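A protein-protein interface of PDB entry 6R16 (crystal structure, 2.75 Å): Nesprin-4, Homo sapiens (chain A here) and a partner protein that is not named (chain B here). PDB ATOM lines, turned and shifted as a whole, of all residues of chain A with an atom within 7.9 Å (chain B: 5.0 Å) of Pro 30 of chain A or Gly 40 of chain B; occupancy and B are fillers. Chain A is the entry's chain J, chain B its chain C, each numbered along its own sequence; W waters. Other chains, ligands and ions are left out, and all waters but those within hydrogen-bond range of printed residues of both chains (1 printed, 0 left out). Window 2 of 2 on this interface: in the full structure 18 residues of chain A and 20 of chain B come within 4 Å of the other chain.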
ATOM      1  N   LEU A  23      -4.513 -19.515  -8.417  1.00  0.00           N
ATOM      2  CA  LEU A  23      -4.492 -20.366  -7.236  1.00  0.00           C
ATOM      3  C   LEU A  23      -3.512 -19.762  -6.238  1.00  0.00           C
ATOM      4  O   LEU A  23      -2.339 -19.551  -6.565  1.00  0.00           O
ATOM      5  CB  LEU A  23      -4.098 -21.801  -7.594  1.00  0.00           C
ATOM      6  CG  LEU A  23      -4.273 -22.894  -6.531  1.00  0.00           C
ATOM      7  CD1 LEU A  23      -4.494 -24.242  -7.194  1.00  0.00           C
ATOM      8  CD2 LEU A  23      -3.079 -22.965  -5.592  1.00  0.00           C
ATOM      9  N   SER A  24      -3.994 -19.485  -5.029  1.00  0.00           N
ATOM     10  CA  SER A  24      -3.161 -18.935  -3.969  1.00  0.00           C
ATOM     11  C   SER A  24      -3.449 -19.677  -2.675  1.00  0.00           C
ATOM     12  O   SER A  24      -4.606 -19.976  -2.367  1.00  0.00           O
ATOM     13  CB  SER A  24      -3.406 -17.433  -3.778  1.00  0.00           C
ATOM     14  OG  SER A  24      -3.093 -16.711  -4.956  1.00  0.00           O
ATOM     15  N   TYR A  25      -2.393 -19.975  -1.925  1.00  0.00           N
ATOM     16  CA  TYR A  25      -2.515 -20.660  -0.646  1.00  0.00           C
ATOM     17  C   TYR A  25      -2.511 -19.622   0.468  1.00  0.00           C
ATOM     18  O   TYR A  25      -1.538 -18.878   0.629  1.00  0.00           O
ATOM     19  CB  TYR A  25      -1.389 -21.676  -0.456  1.00  0.00           C
ATOM     20  CG  TYR A  25      -1.564 -22.917  -1.302  1.00  0.00           C
ATOM     21  CD1 TYR A  25      -2.547 -23.850  -0.997  1.00  0.00           C
ATOM     22  CD2 TYR A  25      -0.750 -23.159  -2.400  1.00  0.00           C
ATOM     23  CE1 TYR A  25      -2.719 -24.984  -1.763  1.00  0.00           C
ATOM     24  CE2 TYR A  25      -0.911 -24.294  -3.171  1.00  0.00           C
ATOM     25  CZ  TYR A  25      -1.899 -25.203  -2.849  1.00  0.00           C
ATOM     26  OH  TYR A  25      -2.071 -26.336  -3.609  1.00  0.00           O
ATOM     27  N   ASN A  27      -3.865 -20.462   3.835  1.00  0.00           N
ATOM     28  CA  ASN A  27      -3.891 -21.099   5.147  1.00  0.00           C
ATOM     29  C   ASN A  27      -2.975 -22.316   5.164  1.00  0.00           C
ATOM     30  O   ASN A  27      -3.338 -23.401   5.624  1.00  0.00           O
ATOM     31  CB  ASN A  27      -5.316 -21.480   5.543  1.00  0.00           C
ATOM     32  CG  ASN A  27      -5.449 -21.780   7.024  1.00  0.00           C
ATOM     33  OD1 ASN A  27      -4.590 -21.410   7.824  1.00  0.00           O
ATOM     34  ND2 ASN A  27      -6.531 -22.454   7.396  1.00  0.00           N
ATOM     35  N   GLY A  28      -1.764 -22.143   4.646  1.00  0.00           N
ATOM     36  CA  GLY A  28      -0.752 -23.173   4.746  1.00  0.00           C
ATOM     37  C   GLY A  28      -0.849 -24.221   3.651  1.00  0.00           C
ATOM     38  O   GLY A  28      -1.403 -24.002   2.568  1.00  0.00           O
ATOM     39  N   LEU A  29      -0.297 -25.397   3.961  1.00  0.00           N
ATOM     40  CA  LEU A  29      -0.154 -26.484   3.008  1.00  0.00           C
ATOM     41  C   LEU A  29      -1.484 -27.195   2.769  1.00  0.00           C
ATOM     42  O   LEU A  29      -2.318 -27.297   3.674  1.00  0.00           O
ATOM     43  CB  LEU A  29       0.880 -27.495   3.497  1.00  0.00           C
ATOM     44  CG  LEU A  29       2.366 -27.132   3.408  1.00  0.00           C
ATOM     45  CD1 LEU A  29       2.784 -26.165   4.510  1.00  0.00           C
ATOM     46  CD2 LEU A  29       3.221 -28.392   3.440  1.00  0.00           C
ATOM     47  N   PRO A  30      -1.705 -27.691   1.555  1.00  0.00           N
ATOM     48  CA  PRO A  30      -2.835 -28.586   1.307  1.00  0.00           C
ATOM     49  C   PRO A  30      -2.505 -29.997   1.757  1.00  0.00           C
ATOM     50  O   PRO A  30      -1.332 -30.317   2.007  1.00  0.00           O
ATOM     51  CB  PRO A  30      -3.009 -28.509  -0.217  1.00  0.00           C
ATOM     52  CG  PRO A  30      -1.633 -28.238  -0.720  1.00  0.00           C
ATOM     53  CD  PRO A  30      -0.976 -27.359   0.318  1.00  0.00           C
ATOM     54  N   PRO A  31      -3.505 -30.868   1.883  1.00  0.00           N
ATOM     55  CA  PRO A  31      -3.229 -32.245   2.319  1.00  0.00           C
ATOM     56  C   PRO A  31      -2.379 -32.994   1.302  1.00  0.00           C
ATOM     57  O   PRO A  31      -2.722 -33.080   0.120  1.00  0.00           O
ATOM     58  CB  PRO A  31      -4.627 -32.860   2.451  1.00  0.00           C
ATOM     59  CG  PRO A  31      -5.546 -31.693   2.612  1.00  0.00           C
ATOM     60  CD  PRO A  31      -4.950 -30.601   1.783  1.00  0.00           C
ATOM     61  N   VAL A  32      -1.259 -33.535   1.773  1.00  0.00           N
ATOM     62  CA  VAL A  32      -0.366 -34.323   0.928  1.00  0.00           C
ATOM     63  C   VAL A  32      -0.121 -35.689   1.561  1.00  0.00           C
ATOM     64  O   VAL A  32      -0.344 -35.885   2.756  1.00  0.00           O
ATOM     65  CB  VAL A  32       0.968 -33.596   0.683  1.00  0.00           C
ATOM     66  CG1 VAL A  32       0.732 -32.265  -0.019  1.00  0.00           C
ATOM     67  CG2 VAL A  32       1.709 -33.395   1.994  1.00  0.00           C
ATOM     68  OXT VAL A  32       0.303 -36.633   0.893  1.00  0.00           O
ATOM     69  N   LEU B  36       6.211 -27.086  -6.519  1.00  0.00           N
ATOM     70  CA  LEU B  36       5.093 -27.765  -7.164  1.00  0.00           C
ATOM     71  C   LEU B  36       3.767 -27.262  -6.610  1.00  0.00           C
ATOM     72  O   LEU B  36       3.567 -27.212  -5.393  1.00  0.00           O
ATOM     73  CB  LEU B  36       5.215 -29.277  -6.959  1.00  0.00           C
ATOM     74  CG  LEU B  36       4.209 -30.177  -7.676  1.00  0.00           C
ATOM     75  CD1 LEU B  36       4.425 -30.137  -9.183  1.00  0.00           C
ATOM     76  CD2 LEU B  36       4.296 -31.600  -7.152  1.00  0.00           C
ATOM     77  N   GLU B  37       2.858 -26.888  -7.515  1.00  0.00           N
ATOM     78  CA  GLU B  37       1.606 -26.265  -7.096  1.00  0.00           C
ATOM     79  C   GLU B  37       0.741 -27.232  -6.295  1.00  0.00           C
ATOM     80  O   GLU B  37       0.228 -26.880  -5.226  1.00  0.00           O
ATOM     81  CB  GLU B  37       0.842 -25.743  -8.313  1.00  0.00           C
ATOM     82  CG  GLU B  37      -0.415 -24.961  -7.959  1.00  0.00           C
ATOM     83  CD  GLU B  37      -1.145 -24.435  -9.180  1.00  0.00           C
ATOM     84  OE1 GLU B  37      -1.600 -25.257 -10.003  1.00  0.00           O
ATOM     85  OE2 GLU B  37      -1.265 -23.199  -9.315  1.00  0.00           O
ATOM     86  N   SER B  38       0.572 -28.458  -6.794  1.00  0.00           N
ATOM     87  CA  SER B  38      -0.271 -29.428  -6.105  1.00  0.00           C
ATOM     88  C   SER B  38       0.269 -29.791  -4.729  1.00  0.00           C
ATOM     89  O   SER B  38      -0.502 -30.219  -3.864  1.00  0.00           O
ATOM     90  CB  SER B  38      -0.427 -30.688  -6.958  1.00  0.00           C
ATOM     91  OG  SER B  38       0.822 -31.324  -7.165  1.00  0.00           O
ATOM     92  N   GLY B  39       1.568 -29.620  -4.500  1.00  0.00           N
ATOM     93  CA  GLY B  39       2.168 -29.924  -3.222  1.00  0.00           C
ATOM     94  C   GLY B  39       2.247 -28.769  -2.255  1.00  0.00           C
ATOM     95  O   GLY B  39       2.740 -28.946  -1.137  1.00  0.00           O
ATOM     96  N   GLY B  40       1.777 -27.585  -2.644  1.00  0.00           N
ATOM     97  CA  GLY B  40       1.787 -26.443  -1.752  1.00  0.00           C
ATOM     98  C   GLY B  40       2.381 -25.185  -2.353  1.00  0.00           C
ATOM     99  O   GLY B  40       2.284 -24.104  -1.764  1.00  0.00           O
ATOM    100  N   GLY B  41       2.996 -25.311  -3.530  1.00  0.00           N
ATOM    101  CA  GLY B  41       3.557 -24.155  -4.192  1.00  0.00           C
ATOM    102  C   GLY B  41       2.498 -23.301  -4.861  1.00  0.00           C
ATOM    103  O   GLY B  41       1.407 -23.760  -5.195  1.00  0.00           O
ATOM    104  N   SER B  42       2.831 -22.027  -5.053  1.00  0.00           N
ATOM    105  CA  SER B  42       1.901 -21.087  -5.662  1.00  0.00           C
ATOM    106  C   SER B  42       2.688 -19.979  -6.346  1.00  0.00           C
ATOM    107  O   SER B  42       3.840 -19.702  -6.002  1.00  0.00           O
ATOM    108  CB  SER B  42       0.930 -20.502  -4.628  1.00  0.00           C
ATOM    109  OG  SER B  42       1.626 -19.934  -3.533  1.00  0.00           O
ATOM    110  N   ARG B  99       6.060 -18.881  -4.526  1.00  0.00           N
ATOM    111  CA  ARG B  99       6.022 -19.092  -3.084  1.00  0.00           C
ATOM    112  C   ARG B  99       6.164 -20.583  -2.803  1.00  0.00           C
ATOM    113  O   ARG B  99       5.307 -21.379  -3.204  1.00  0.00           O
ATOM    114  CB  ARG B  99       4.726 -18.550  -2.483  1.00  0.00           C
ATOM    115  CG  ARG B  99       4.655 -18.697  -0.971  1.00  0.00           C
ATOM    116  CD  ARG B  99       3.301 -18.279  -0.426  1.00  0.00           C
ATOM    117  NE  ARG B  99       3.257 -18.369   1.031  1.00  0.00           N
ATOM    118  CZ  ARG B  99       2.969 -19.480   1.703  1.00  0.00           C
ATOM    119  NH1 ARG B  99       2.697 -20.602   1.050  1.00  0.00           N
ATOM    120  NH2 ARG B  99       2.953 -19.468   3.029  1.00  0.00           N
ATOM    121  N   LEU B 100       7.244 -20.958  -2.125  1.00  0.00           N
ATOM    122  CA  LEU B 100       7.512 -22.359  -1.851  1.00  0.00           C
ATOM    123  C   LEU B 100       6.508 -22.920  -0.848  1.00  0.00           C
ATOM    124  O   LEU B 100       5.868 -22.190  -0.086  1.00  0.00           O
ATOM    125  CB  LEU B 100       8.935 -22.541  -1.327  1.00  0.00           C
ATOM    126  CG  LEU B 100      10.034 -22.060  -2.274  1.00  0.00           C
ATOM    127  CD1 LEU B 100      11.408 -22.381  -1.712  1.00  0.00           C
ATOM    128  CD2 LEU B 100       9.853 -22.680  -3.649  1.00  0.00           C
ATOM    129  N   SER B 101       6.378 -24.249  -0.860  1.00  0.00           N
ATOM    130  CA  SER B 101       5.435 -24.906   0.038  1.00  0.00           C
ATOM    131  C   SER B 101       5.906 -24.858   1.484  1.00  0.00           C
ATOM    132  O   SER B 101       5.078 -24.859   2.403  1.00  0.00           O
ATOM    133  CB  SER B 101       5.209 -26.352  -0.403  1.00  0.00           C
ATOM    134  OG  SER B 101       6.411 -27.098  -0.345  1.00  0.00           O
HETATM  135  O   HOH W   1      -0.195 -20.660  -8.188  1.00  0.00           O
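The side-chain hydroxyl (OH) of Tyr 25 of chain A sits at hydrogen-bond distance from the backbone carbonyl oxygen (O) of Glu 37 of chain B, at 2.9 Å.
The backbone carbonyl oxygen (O) of Leu 36 of chain B is in hydrogen-bond range of the backbone NH (N) of Gly 41 of chain B. The backbone NH (N) of Arg 99 of chain B sits at hydrogen-bond distance from the backbone carbonyl oxygen (O) of Ser 42 of chain B, at 2.8 Å.
OE2 of Glu 37 of chain B touches CB of Leu 23 of chain A, 3.6 Å away. Leu 23 of chain A touches Ser 42 of chain B. CD2 of Tyr 25 of chain A touches O of Gly 40 of chain B, at 3.2 Å. Tyr 25 of chain A touches Gly 41 of chain B. Tyr 25 of chain A touches Ser 42 of chain B. Ser 101 of chain B touches Leu 29 of chain A (O to CD1, 3.4 Å). Ser 38 of chain B touches Pro 30 of chain A. Pro 30 of chain A touches Gly 40 of chain B (CD to CA, 3.6 Å).
Of chain B, only Ser 38 and Gly 40 come within 4 Å of Pro 30 of chain A. Gly 41 of chain B touches just one residue of chain A: Tyr 25. Printed residues of chain A within 4 Å of Glu 37 of chain B: Leu 23 and Tyr 25. Of the printed residues of chain A, Ser 101 of chain B touches Leu 29 (3.4 Å). Printed residues of chain A within 4 Å of Ser 38 of chain B: Pro 30 (3.9 Å). Of the printed residues of chain B, Tyr 25 of chain A touches Glu 37 (2.9 Å), Gly 40 (3.2 Å), Gly 41 (3.1 Å) and Ser 42 (3.9 Å). Leu 100 of chain B touches none of the printed residues of chain A. Pro 31 of chain A touches none of the printed residues of chain B. The nearest residue of chain A that does not touch Gly 40 of chain B is Leu 29 of chain A (5.1 Å). The nearest printed residue of chain A that does not touch Ser 38 of chain B is Tyr 25 of chain A (4.2 Å).
Printed residues of chain A that touch a printed residue of chain B: Leu 23, Tyr 25, Leu 29 and Pro 30. Among the printed residues, 9 pairs touch across the chains.
Water W1 bridges the backbone carbonyl oxygen (O) of Leu 23 of chain A (2.9 Å) and the side-chain carboxylate (OE2) of Glu 37 of chain B (3.0 Å).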
